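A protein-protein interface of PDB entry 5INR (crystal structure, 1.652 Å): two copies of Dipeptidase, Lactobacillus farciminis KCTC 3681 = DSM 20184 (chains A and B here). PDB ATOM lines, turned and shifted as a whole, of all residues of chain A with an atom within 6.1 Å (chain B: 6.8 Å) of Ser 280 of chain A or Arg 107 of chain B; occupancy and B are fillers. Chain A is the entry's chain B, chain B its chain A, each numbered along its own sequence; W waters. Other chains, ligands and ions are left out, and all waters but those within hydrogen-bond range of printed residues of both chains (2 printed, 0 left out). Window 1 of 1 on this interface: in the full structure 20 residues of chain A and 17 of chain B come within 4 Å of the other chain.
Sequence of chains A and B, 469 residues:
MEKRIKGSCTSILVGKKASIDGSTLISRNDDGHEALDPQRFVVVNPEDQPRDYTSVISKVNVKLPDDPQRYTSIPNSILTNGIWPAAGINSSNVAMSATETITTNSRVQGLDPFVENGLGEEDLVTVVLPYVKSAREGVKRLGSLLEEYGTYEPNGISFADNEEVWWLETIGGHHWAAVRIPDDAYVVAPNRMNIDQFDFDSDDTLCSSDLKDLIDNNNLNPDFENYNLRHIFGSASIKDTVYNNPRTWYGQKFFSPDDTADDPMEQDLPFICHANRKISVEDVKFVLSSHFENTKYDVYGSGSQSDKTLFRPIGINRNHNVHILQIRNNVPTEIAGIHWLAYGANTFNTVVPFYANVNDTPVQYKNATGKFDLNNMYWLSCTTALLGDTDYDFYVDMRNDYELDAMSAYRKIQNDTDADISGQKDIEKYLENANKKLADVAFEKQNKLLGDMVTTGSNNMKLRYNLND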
ATOM      1  N   ALA A  18       1.860   6.047 -29.299  1.00  0.00           N
ATOM      2  CA  ALA A  18       1.309   5.089 -30.255  1.00  0.00           C
ATOM      3  C   ALA A  18      -0.172   4.785 -29.992  1.00  0.00           C
ATOM      4  O   ALA A  18      -0.870   4.232 -30.853  1.00  0.00           O
ATOM      5  CB  ALA A  18       2.115   3.808 -30.224  1.00  0.00           C
ATOM      6  N   SER A  19      -0.640   5.133 -28.801  1.00  0.00           N
ATOM      7  CA  SER A  19      -2.029   4.904 -28.402  1.00  0.00           C
ATOM      8  C   SER A  19      -2.923   6.040 -28.865  1.00  0.00           C
ATOM      9  O   SER A  19      -2.467   7.166 -29.062  1.00  0.00           O
ATOM     10  CB  SER A  19      -2.137   4.769 -26.889  1.00  0.00           C
ATOM     11  OG  SER A  19      -1.656   5.963 -26.279  1.00  0.00           O
ATOM     12  N   ILE A  20      -4.214   5.758 -28.998  1.00  0.00           N
ATOM     13  CA  ILE A  20      -5.127   6.769 -29.508  1.00  0.00           C
ATOM     14  C   ILE A  20      -5.345   7.895 -28.490  1.00  0.00           C
ATOM     15  O   ILE A  20      -5.702   9.014 -28.868  1.00  0.00           O
ATOM     16  CB  ILE A  20      -6.481   6.143 -29.898  1.00  0.00           C
ATOM     17  CG1 ILE A  20      -7.295   7.106 -30.767  1.00  0.00           C
ATOM     18  CG2 ILE A  20      -7.257   5.701 -28.659  1.00  0.00           C
ATOM     19  CD1 ILE A  20      -8.549   6.451 -31.392  1.00  0.00           C
ATOM     20  N   LEU A  25      -0.004   1.228 -22.687  1.00  0.00           N
ATOM     21  CA  LEU A  25      -0.731  -0.026 -22.559  1.00  0.00           C
ATOM     22  C   LEU A  25       0.238  -1.191 -22.507  1.00  0.00           C
ATOM     23  O   LEU A  25       1.148  -1.287 -23.337  1.00  0.00           O
ATOM     24  CB  LEU A  25      -1.692  -0.242 -23.740  1.00  0.00           C
ATOM     25  CG  LEU A  25      -2.735   0.813 -24.097  1.00  0.00           C
ATOM     26  CD1 LEU A  25      -3.355   0.479 -25.459  1.00  0.00           C
ATOM     27  CD2 LEU A  25      -3.809   0.880 -23.030  1.00  0.00           C
ATOM     28  N   PHE A 255      -1.732  -4.151 -37.540  1.00  0.00           N
ATOM     29  CA  PHE A 255      -1.272  -2.798 -37.199  1.00  0.00           C
ATOM     30  C   PHE A 255      -0.347  -2.171 -38.244  1.00  0.00           C
ATOM     31  O   PHE A 255      -0.342  -0.945 -38.416  1.00  0.00           O
ATOM     32  CB  PHE A 255      -0.546  -2.807 -35.847  1.00  0.00           C
ATOM     33  CG  PHE A 255      -1.460  -3.000 -34.675  1.00  0.00           C
ATOM     34  CD1 PHE A 255      -2.523  -2.139 -34.469  1.00  0.00           C
ATOM     35  CD2 PHE A 255      -1.255  -4.044 -33.778  1.00  0.00           C
ATOM     36  CE1 PHE A 255      -3.378  -2.312 -33.389  1.00  0.00           C
ATOM     37  CE2 PHE A 255      -2.101  -4.218 -32.689  1.00  0.00           C
ATOM     38  CZ  PHE A 255      -3.168  -3.356 -32.498  1.00  0.00           C
ATOM     39  N   LYS A 278      -2.954   5.203 -34.776  1.00  0.00           N
ATOM     40  CA  LYS A 278      -2.902   5.076 -33.330  1.00  0.00           C
ATOM     41  C   LYS A 278      -3.779   3.918 -32.862  1.00  0.00           C
ATOM     42  O   LYS A 278      -4.758   3.567 -33.518  1.00  0.00           O
ATOM     43  CB  LYS A 278      -3.341   6.371 -32.653  1.00  0.00           C
ATOM     44  CG  LYS A 278      -2.500   7.578 -33.053  1.00  0.00           C
ATOM     45  CD  LYS A 278      -3.091   8.835 -32.406  1.00  0.00           C
ATOM     46  CE  LYS A 278      -2.403  10.101 -32.870  1.00  0.00           C
ATOM     47  NZ  LYS A 278      -3.029  11.282 -32.192  1.00  0.00           N
ATOM     48  N   ILE A 279      -3.412   3.330 -31.727  1.00  0.00           N
ATOM     49  CA  ILE A 279      -3.991   2.071 -31.259  1.00  0.00           C
ATOM     50  C   ILE A 279      -4.962   2.250 -30.087  1.00  0.00           C
ATOM     51  O   ILE A 279      -4.658   2.942 -29.116  1.00  0.00           O
ATOM     52  CB  ILE A 279      -2.855   1.100 -30.853  1.00  0.00           C
ATOM     53  CG1 ILE A 279      -1.962   0.826 -32.074  1.00  0.00           C
ATOM     54  CG2 ILE A 279      -3.408  -0.181 -30.195  1.00  0.00           C
ATOM     55  CD1 ILE A 279      -0.672   0.087 -31.761  1.00  0.00           C
ATOM     56  N   SER A 280      -6.136   1.630 -30.191  1.00  0.00           N
ATOM     57  CA  SER A 280      -7.156   1.706 -29.150  1.00  0.00           C
ATOM     58  C   SER A 280      -7.162   0.451 -28.299  1.00  0.00           C
ATOM     59  O   SER A 280      -6.590  -0.576 -28.679  1.00  0.00           O
ATOM     60  CB  SER A 280      -8.540   1.910 -29.770  1.00  0.00           C
ATOM     61  OG  SER A 280      -8.924   0.734 -30.470  1.00  0.00           O
ATOM     62  N   VAL A 281      -7.829   0.527 -27.158  1.00  0.00           N
ATOM     63  CA  VAL A 281      -8.009  -0.642 -26.319  1.00  0.00           C
ATOM     64  C   VAL A 281      -8.789  -1.684 -27.120  1.00  0.00           C
ATOM     65  O   VAL A 281      -8.462  -2.869 -27.079  1.00  0.00           O
ATOM     66  CB  VAL A 281      -8.741  -0.299 -25.001  1.00  0.00           C
ATOM     67  CG1 VAL A 281      -9.179  -1.556 -24.269  1.00  0.00           C
ATOM     68  CG2 VAL A 281      -7.831   0.544 -24.096  1.00  0.00           C
ATOM     69  N   GLU A 282      -9.787  -1.224 -27.871  1.00  0.00           N
ATOM     70  CA  GLU A 282     -10.562  -2.117 -28.733  1.00  0.00           C
ATOM     71  C   GLU A 282      -9.665  -2.879 -29.719  1.00  0.00           C
ATOM     72  O   GLU A 282      -9.864  -4.083 -29.919  1.00  0.00           O
ATOM     73  CB  GLU A 282     -11.628  -1.333 -29.495  1.00  0.00           C
ATOM     74  CG  GLU A 282     -12.847  -0.910 -28.653  1.00  0.00           C
ATOM     75  CD  GLU A 282     -12.650   0.377 -27.836  1.00  0.00           C
ATOM     76  OE1 GLU A 282     -11.557   1.019 -27.870  1.00  0.00           O
ATOM     77  OE2 GLU A 282     -13.633   0.756 -27.151  1.00  0.00           O
ATOM     78  N   ASP A 283      -8.692  -2.190 -30.325  1.00  0.00           N
ATOM     79  CA  ASP A 283      -7.712  -2.831 -31.221  1.00  0.00           C
ATOM     80  C   ASP A 283      -6.935  -3.940 -30.515  1.00  0.00           C
ATOM     81  O   ASP A 283      -6.748  -5.037 -31.053  1.00  0.00           O
ATOM     82  CB  ASP A 283      -6.692  -1.821 -31.758  1.00  0.00           C
ATOM     83  CG  ASP A 283      -7.287  -0.805 -32.713  1.00  0.00           C
ATOM     84  OD1 ASP A 283      -8.316  -1.084 -33.368  1.00  0.00           O
ATOM     85  OD2 ASP A 283      -6.685   0.287 -32.826  1.00  0.00           O
ATOM     86  N   VAL A 284      -6.440  -3.633 -29.319  1.00  0.00           N
ATOM     87  CA  VAL A 284      -5.635  -4.589 -28.585  1.00  0.00           C
ATOM     88  C   VAL A 284      -6.482  -5.820 -28.269  1.00  0.00           C
ATOM     89  O   VAL A 284      -6.037  -6.948 -28.485  1.00  0.00           O
ATOM     90  CB  VAL A 284      -5.062  -3.963 -27.302  1.00  0.00           C
ATOM     91  CG1 VAL A 284      -4.362  -5.015 -26.466  1.00  0.00           C
ATOM     92  CG2 VAL A 284      -4.092  -2.846 -27.684  1.00  0.00           C
ATOM     93  N   LYS A 285      -7.706  -5.617 -27.789  1.00  0.00           N
ATOM     94  CA  LYS A 285      -8.562  -6.760 -27.453  1.00  0.00           C
ATOM     95  C   LYS A 285      -8.869  -7.581 -28.705  1.00  0.00           C
ATOM     96  O   LYS A 285      -8.894  -8.816 -28.644  1.00  0.00           O
ATOM     97  CB  LYS A 285      -9.858  -6.297 -26.762  1.00  0.00           C
ATOM     98  CG  LYS A 285     -10.872  -7.414 -26.425  1.00  0.00           C
ATOM     99  CD  LYS A 285     -10.258  -8.518 -25.549  1.00  0.00           C
ATOM    100  CE  LYS A 285     -11.335  -9.414 -24.918  1.00  0.00           C
ATOM    101  NZ  LYS A 285     -12.238 -10.069 -25.936  1.00  0.00           N
ATOM    102  N   SER A 408     -19.570   0.072 -25.382  1.00  0.00           N
ATOM    103  CA  SER A 408     -20.184   1.399 -25.375  1.00  0.00           C
ATOM    104  C   SER A 408     -20.659   1.763 -23.976  1.00  0.00           C
ATOM    105  O   SER A 408     -20.451   2.886 -23.506  1.00  0.00           O
ATOM    106  CB  SER A 408     -21.364   1.456 -26.354  1.00  0.00           C
ATOM    107  OG  SER A 408     -20.918   1.296 -27.687  1.00  0.00           O
ATOM    108  N   ARG A 411     -17.705   2.540 -21.634  1.00  0.00           N
ATOM    109  CA  ARG A 411     -17.075   3.832 -21.884  1.00  0.00           C
ATOM    110  C   ARG A 411     -17.969   4.978 -21.406  1.00  0.00           C
ATOM    111  O   ARG A 411     -17.468   6.016 -20.973  1.00  0.00           O
ATOM    112  CB  ARG A 411     -16.711   3.985 -23.359  1.00  0.00           C
ATOM    113  CG  ARG A 411     -15.496   3.122 -23.753  1.00  0.00           C
ATOM    114  CD  ARG A 411     -14.843   3.617 -25.027  1.00  0.00           C
ATOM    115  NE  ARG A 411     -13.605   2.913 -25.370  1.00  0.00           N
ATOM    116  CZ  ARG A 411     -12.409   3.183 -24.847  1.00  0.00           C
ATOM    117  NH1 ARG A 411     -12.279   4.128 -23.924  1.00  0.00           N
ATOM    118  NH2 ARG A 411     -11.335   2.506 -25.248  1.00  0.00           N
ATOM    119  N   ASN A 415     -16.541   7.634 -18.889  1.00  0.00           N
ATOM    120  CA  ASN A 415     -16.606   9.056 -19.223  1.00  0.00           C
ATOM    121  C   ASN A 415     -17.384   9.855 -18.174  1.00  0.00           C
ATOM    122  O   ASN A 415     -16.989  10.968 -17.817  1.00  0.00           O
ATOM    123  CB  ASN A 415     -17.228   9.254 -20.611  1.00  0.00           C
ATOM    124  CG  ASN A 415     -16.337   8.735 -21.736  1.00  0.00           C
ATOM    125  OD1 ASN A 415     -15.112   8.675 -21.601  1.00  0.00           O
ATOM    126  ND2 ASN A 415     -16.959   8.336 -22.850  1.00  0.00           N
ATOM    127  N   THR B 104     -20.985   2.226 -36.339  1.00  0.00           N
ATOM    128  CA  THR B 104     -20.527   3.189 -35.345  1.00  0.00           C
ATOM    129  C   THR B 104     -19.409   2.504 -34.554  1.00  0.00           C
ATOM    130  O   THR B 104     -18.910   1.455 -34.976  1.00  0.00           O
ATOM    131  CB  THR B 104     -21.712   3.656 -34.453  1.00  0.00           C
ATOM    132  OG1 THR B 104     -21.294   4.703 -33.565  1.00  0.00           O
ATOM    133  CG2 THR B 104     -22.285   2.504 -33.636  1.00  0.00           C
ATOM    134  N   ASN B 105     -18.969   3.091 -33.446  1.00  0.00           N
ATOM    135  CA  ASN B 105     -18.024   2.392 -32.571  1.00  0.00           C
ATOM    136  C   ASN B 105     -18.212   2.818 -31.121  1.00  0.00           C
ATOM    137  O   ASN B 105     -18.947   3.764 -30.828  1.00  0.00           O
ATOM    138  CB  ASN B 105     -16.567   2.588 -33.037  1.00  0.00           C
ATOM    139  CG  ASN B 105     -16.084   4.033 -32.939  1.00  0.00           C
ATOM    140  OD1 ASN B 105     -16.065   4.621 -31.854  1.00  0.00           O
ATOM    141  ND2 ASN B 105     -15.641   4.591 -34.067  1.00  0.00           N
ATOM    142  N   SER B 106     -17.576   2.090 -30.212  1.00  0.00           N
ATOM    143  CA  SER B 106     -17.831   2.257 -28.793  1.00  0.00           C
ATOM    144  C   SER B 106     -17.267   3.549 -28.225  1.00  0.00           C
ATOM    145  O   SER B 106     -17.757   4.038 -27.207  1.00  0.00           O
ATOM    146  CB  SER B 106     -17.261   1.075 -28.018  1.00  0.00           C
ATOM    147  OG  SER B 106     -15.927   0.803 -28.412  1.00  0.00           O
ATOM    148  N   ARG B 107     -16.243   4.096 -28.869  1.00  0.00           N
ATOM    149  CA  ARG B 107     -15.640   5.327 -28.369  1.00  0.00           C
ATOM    150  C   ARG B 107     -16.595   6.500 -28.565  1.00  0.00           C
ATOM    151  O   ARG B 107     -16.819   7.282 -27.628  1.00  0.00           O
ATOM    152  CB  ARG B 107     -14.288   5.578 -29.050  1.00  0.00           C
ATOM    153  CG  ARG B 107     -13.212   4.567 -28.622  1.00  0.00           C
ATOM    154  CD  ARG B 107     -11.939   4.621 -29.482  1.00  0.00           C
ATOM    155  NE  ARG B 107     -12.221   4.335 -30.884  1.00  0.00           N
ATOM    156  CZ  ARG B 107     -12.471   3.120 -31.364  1.00  0.00           C
ATOM    157  NH1 ARG B 107     -12.438   2.064 -30.558  1.00  0.00           N
ATOM    158  NH2 ARG B 107     -12.742   2.958 -32.654  1.00  0.00           N
ATOM    159  N   VAL B 108     -17.213   6.617 -29.737  1.00  0.00           N
ATOM    160  CA  VAL B 108     -18.159   7.719 -29.910  1.00  0.00           C
ATOM    161  C   VAL B 108     -19.479   7.436 -29.182  1.00  0.00           C
ATOM    162  O   VAL B 108     -20.086   8.363 -28.630  1.00  0.00           O
ATOM    163  CB  VAL B 108     -18.427   8.050 -31.404  1.00  0.00           C
ATOM    164  CG1 VAL B 108     -18.988   6.853 -32.163  1.00  0.00           C
ATOM    165  CG2 VAL B 108     -19.340   9.288 -31.541  1.00  0.00           C
ATOM    166  N   GLN B 109     -19.914   6.173 -29.134  1.00  0.00           N
ATOM    167  CA  GLN B 109     -21.149   5.850 -28.423  1.00  0.00           C
ATOM    168  C   GLN B 109     -21.034   6.121 -26.928  1.00  0.00           C
ATOM    169  O   GLN B 109     -22.022   6.459 -26.280  1.00  0.00           O
ATOM    170  CB  GLN B 109     -21.561   4.384 -28.650  1.00  0.00           C
ATOM    171  CG  GLN B 109     -22.053   4.096 -30.071  1.00  0.00           C
ATOM    172  CD  GLN B 109     -23.370   4.797 -30.388  1.00  0.00           C
ATOM    173  OE1 GLN B 109     -24.232   4.939 -29.523  1.00  0.00           O
ATOM    174  NE2 GLN B 109     -23.512   5.263 -31.625  1.00  0.00           N
ATOM    175  N   GLY B 110     -19.827   5.982 -26.391  1.00  0.00           N
ATOM    176  CA  GLY B 110     -19.585   6.263 -24.991  1.00  0.00           C
ATOM    177  C   GLY B 110     -19.721   7.742 -24.660  1.00  0.00           C
ATOM    178  O   GLY B 110     -19.956   8.096 -23.501  1.00  0.00           O
ATOM    179  N   LEU B 111     -19.597   8.599 -25.676  1.00  0.00           N
ATOM    180  CA  LEU B 111     -19.687  10.055 -25.490  1.00  0.00           C
ATOM    181  C   LEU B 111     -21.060  10.632 -25.823  1.00  0.00           C
ATOM    182  O   LEU B 111     -21.498  11.604 -25.206  1.00  0.00           O
ATOM    183  CB  LEU B 111     -18.641  10.761 -26.354  1.00  0.00           C
ATOM    184  CG  LEU B 111     -17.183  10.583 -25.941  1.00  0.00           C
ATOM    185  CD1 LEU B 111     -16.264  11.076 -27.046  1.00  0.00           C
ATOM    186  CD2 LEU B 111     -16.905  11.332 -24.633  1.00  0.00           C
ATOM    187  N   ASP B 112     -21.716  10.047 -26.822  1.00  0.00           N
ATOM    188  CA  ASP B 112     -23.012  10.519 -27.306  1.00  0.00           C
ATOM    189  C   ASP B 112     -23.875   9.303 -27.619  1.00  0.00           C
ATOM    190  O   ASP B 112     -24.040   8.930 -28.783  1.00  0.00           O
ATOM    191  CB  ASP B 112     -22.829  11.400 -28.545  1.00  0.00           C
ATOM    192  CG  ASP B 112     -24.138  11.950 -29.088  1.00  0.00           C
ATOM    193  OD1 ASP B 112     -25.170  11.903 -28.375  1.00  0.00           O
ATOM    194  OD2 ASP B 112     -24.129  12.434 -30.238  1.00  0.00           O
ATOM    195  N   ASN B 218     -11.535  14.686 -27.331  1.00  0.00           N
ATOM    196  CA  ASN B 218     -11.816  13.399 -26.709  1.00  0.00           C
ATOM    197  C   ASN B 218     -10.994  12.244 -27.279  1.00  0.00           C
ATOM    198  O   ASN B 218     -11.361  11.079 -27.116  1.00  0.00           O
ATOM    199  CB  ASN B 218     -13.311  13.091 -26.818  1.00  0.00           C
ATOM    200  CG  ASN B 218     -14.166  14.090 -26.032  1.00  0.00           C
ATOM    201  OD1 ASN B 218     -14.244  14.018 -24.806  1.00  0.00           O
ATOM    202  ND2 ASN B 218     -14.796  15.024 -26.738  1.00  0.00           N
ATOM    203  N   ASN B 219      -9.882  12.587 -27.924  1.00  0.00           N
ATOM    204  CA  ASN B 219      -8.934  11.597 -28.422  1.00  0.00           C
ATOM    205  C   ASN B 219      -9.598  10.583 -29.330  1.00  0.00           C
ATOM    206  O   ASN B 219      -9.327   9.388 -29.217  1.00  0.00           O
ATOM    207  CB  ASN B 219      -8.278  10.860 -27.247  1.00  0.00           C
ATOM    208  CG  ASN B 219      -7.432  11.767 -26.379  1.00  0.00           C
ATOM    209  OD1 ASN B 219      -6.561  12.478 -26.873  1.00  0.00           O
ATOM    210  ND2 ASN B 219      -7.712  11.773 -25.079  1.00  0.00           N
ATOM    211  N   LEU B 220     -10.495  11.047 -30.199  1.00  0.00           N
ATOM    212  CA  LEU B 220     -11.232  10.122 -31.068  1.00  0.00           C
ATOM    213  C   LEU B 220     -10.498   9.792 -32.361  1.00  0.00           C
ATOM    214  O   LEU B 220     -10.840   8.821 -33.040  1.00  0.00           O
ATOM    215  CB  LEU B 220     -12.613  10.685 -31.421  1.00  0.00           C
ATOM    216  CG  LEU B 220     -13.605  10.838 -30.268  1.00  0.00           C
ATOM    217  CD1 LEU B 220     -14.957  11.322 -30.790  1.00  0.00           C
ATOM    218  CD2 LEU B 220     -13.765   9.530 -29.508  1.00  0.00           C
ATOM    219  N   PRO B 222      -7.923   8.359 -34.773  1.00  0.00           N
ATOM    220  CA  PRO B 222      -6.875   7.340 -34.785  1.00  0.00           C
ATOM    221  C   PRO B 222      -5.734   7.659 -35.731  1.00  0.00           C
ATOM    222  O   PRO B 222      -4.704   6.976 -35.698  1.00  0.00           O
ATOM    223  CB  PRO B 222      -7.623   6.085 -35.251  1.00  0.00           C
ATOM    224  CG  PRO B 222      -8.663   6.618 -36.171  1.00  0.00           C
ATOM    225  CD  PRO B 222      -9.094   7.961 -35.575  1.00  0.00           C
ATOM    226  N   HIS B 231     -12.982   6.414 -40.157  1.00  0.00           N
ATOM    227  CA  HIS B 231     -11.901   5.992 -39.270  1.00  0.00           C
ATOM    228  C   HIS B 231     -12.190   6.396 -37.827  1.00  0.00           C
ATOM    229  O   HIS B 231     -11.929   5.648 -36.888  1.00  0.00           O
ATOM    230  CB  HIS B 231     -10.563   6.597 -39.693  1.00  0.00           C
ATOM    231  CG  HIS B 231      -9.958   5.955 -40.895  1.00  0.00           C
ATOM    232  ND1 HIS B 231      -8.697   6.274 -41.348  1.00  0.00           N
ATOM    233  CD2 HIS B 231     -10.438   5.016 -41.746  1.00  0.00           C
ATOM    234  CE1 HIS B 231      -8.424   5.555 -42.425  1.00  0.00           C
ATOM    235  NE2 HIS B 231      -9.464   4.783 -42.684  1.00  0.00           N
ATOM    236  N   ILE B 232     -12.748   7.592 -37.670  1.00  0.00           N
ATOM    237  CA  ILE B 232     -13.005   8.181 -36.360  1.00  0.00           C
ATOM    238  C   ILE B 232     -14.282   7.649 -35.713  1.00  0.00           C
ATOM    239  O   ILE B 232     -14.279   7.261 -34.541  1.00  0.00           O
ATOM    240  CB  ILE B 232     -13.091   9.727 -36.481  1.00  0.00           C
ATOM    241  CG1 ILE B 232     -11.745  10.282 -36.969  1.00  0.00           C
ATOM    242  CG2 ILE B 232     -13.515  10.361 -35.142  1.00  0.00           C
ATOM    243  CD1 ILE B 232     -11.802  11.726 -37.486  1.00  0.00           C
ATOM    244  N   PHE B 233     -15.357   7.595 -36.499  1.00  0.00           N
ATOM    245  CA  PHE B 233     -16.702   7.357 -35.982  1.00  0.00           C
ATOM    246  C   PHE B 233     -17.311   6.031 -36.426  1.00  0.00           C
ATOM    247  O   PHE B 233     -18.383   5.643 -35.954  1.00  0.00           O
ATOM    248  CB  PHE B 233     -17.630   8.477 -36.432  1.00  0.00           C
ATOM    249  CG  PHE B 233     -17.317   9.818 -35.827  1.00  0.00           C
ATOM    250  CD1 PHE B 233     -17.330   9.990 -34.453  1.00  0.00           C
ATOM    251  CD2 PHE B 233     -17.082  10.911 -36.640  1.00  0.00           C
ATOM    252  CE1 PHE B 233     -17.078  11.245 -33.891  1.00  0.00           C
ATOM    253  CE2 PHE B 233     -16.831  12.164 -36.087  1.00  0.00           C
ATOM    254  CZ  PHE B 233     -16.840  12.325 -34.714  1.00  0.00           C
ATOM    255  N   GLY B 234     -16.634   5.348 -37.343  1.00  0.00           N
ATOM    256  CA  GLY B 234     -17.226   4.172 -37.961  1.00  0.00           C
ATOM    257  C   GLY B 234     -16.522   2.895 -37.563  1.00  0.00           C
ATOM    258  O   GLY B 234     -15.942   2.793 -36.484  1.00  0.00           O
HETATM  259  O   HOH W   1     -15.711   7.262 -25.156  1.00  0.00           O
HETATM  260  O   HOH W   2     -10.285   0.800 -32.826  1.00  0.00           O
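Of the 17 printed residues of chain B, 8 touch a printed residue of chain A.
Hydrophobic or aromatic side chains of chain B that line the printed part of chain A: Leu 111 and Pro 222.
Of the 16 printed residues of chain A, 7 touch a printed residue of chain B.
Among the printed residues, 14 pairs touch across the chains.
Among the printed residues, Asp or Glu carboxylates within 4 Å of a Lys or Arg side-chain nitrogen of the other chain: Glu 282 of chain A with Arg 107 of chain B (3.0 Å).
Of chain B, only Arg 107 (3.8 Å) comes within 4 Å of Ser 280 of chain A.
Of chain A, only Ser 280 (3.8 Å), Glu 282 (3.0 Å) and Arg 411 (3.7 Å) come within 4 Å of Arg 107 of chain B.
Of the printed residues of chain B, Asn 415 of chain A touches Gly 110 (3.1 Å) and Leu 111 (3.5 Å).
Of the printed residues of chain B, Glu 282 of chain A touches Ser 106 and Arg 107.
Printed residues of chain A within 4 Å of Asn 219 of chain B: Ile 20 (3.4 Å).
Printed residues of chain A within 4 Å of Leu 111 of chain B: Asn 415.
Ile 232 of chain B touches none of the printed residues of chain A.
The nearest printed residue of chain B that does not touch Ser 280 of chain A is Pro 222 of chain B (6.9 Å).
The nearest residue of chain A that does not touch Arg 107 of chain B is Ile 20 of chain A (4.3 Å).
The nearest printed residue of chain B that does not touch Glu 282 of chain A is Asn 105 of chain B (6.4 Å).
Among the printed residues, merely in contact across the chains: Ser 408 of chain A with Gln 109 of chain B (3.3 Å), Ser 408 of chain A with Ser 106 of chain B (3.4 Å), Ile 20 of chain A with Asn 219 of chain B (3.4 Å), Asn 415 of chain A with Leu 111 of chain B (3.5 Å), Arg 411 of chain A with Ser 106 of chain B (3.7 Å), Arg 411 of chain A with Arg 107 of chain B (3.7 Å), Ile 20 of chain A with Leu 220 of chain B (3.7 Å), Ser 280 of chain A with Arg 107 of chain B (3.8 Å), Ser 408 of chain A with Gly 110 of chain B (3.8 Å) and Ile 20 of chain A with Pro 222 of chain B (3.9 Å).
OG1 of Thr 104 of chain B is in hydrogen-bond range of NE2 of Gln 109 of chain B (3.0 Å).
N of Arg 107 of chain B is in hydrogen-bond range of OD1 of Asn 105 of chain B, at 3.0 Å.
The backbone carbonyl oxygen (O) of Ile 279 of chain A is in hydrogen-bond range of the backbone NH (N) of Ile 20 of chain A, 2.9 Å away.
OG of Ser 280 of chain A sits close to N of Glu 282 of chain A.
The side-chain hydroxyl (OG) of Ser 280 of chain A lies within hydrogen-bond range of the backbone NH (N) of Asp 283 of chain A, at 2.9 Å.
OE2 of Glu 282 of chain A lies within salt-bridge range of NE of Arg 411 of chain A, 2.8 Å away.
Water W1 bridges O of Arg 107 of chain B (2.7 Å) and ND2 of Asn 415 of chain A (2.8 Å).
Water W2 lies within hydrogen-bond range of OG of Ser 280 of chain A, OD1 of Asp 283 of chain A and NH2 of Arg 107 of chain B.
OE2 of Glu 282 of chain A sits at hydrogen-bond distance from OG of Ser 106 of chain B (2.6 Å).
The guanidinium group of Arg 107 of chain B is in salt-bridge range of the side-chain carboxylate of Glu 282 of chain A, at 3.0 Å.
The backbone carbonyl oxygen (O) of Gly 110 of chain B sits at hydrogen-bond distance from the side-chain amide nitrogen (ND2) of Asn 415 of chain A.
The backbone NH (N) of Lys 278 of chain A lies within hydrogen-bond range of the backbone carbonyl oxygen (O) of Pro 222 of chain B (2.7 Å).
No position is printed for both chains.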
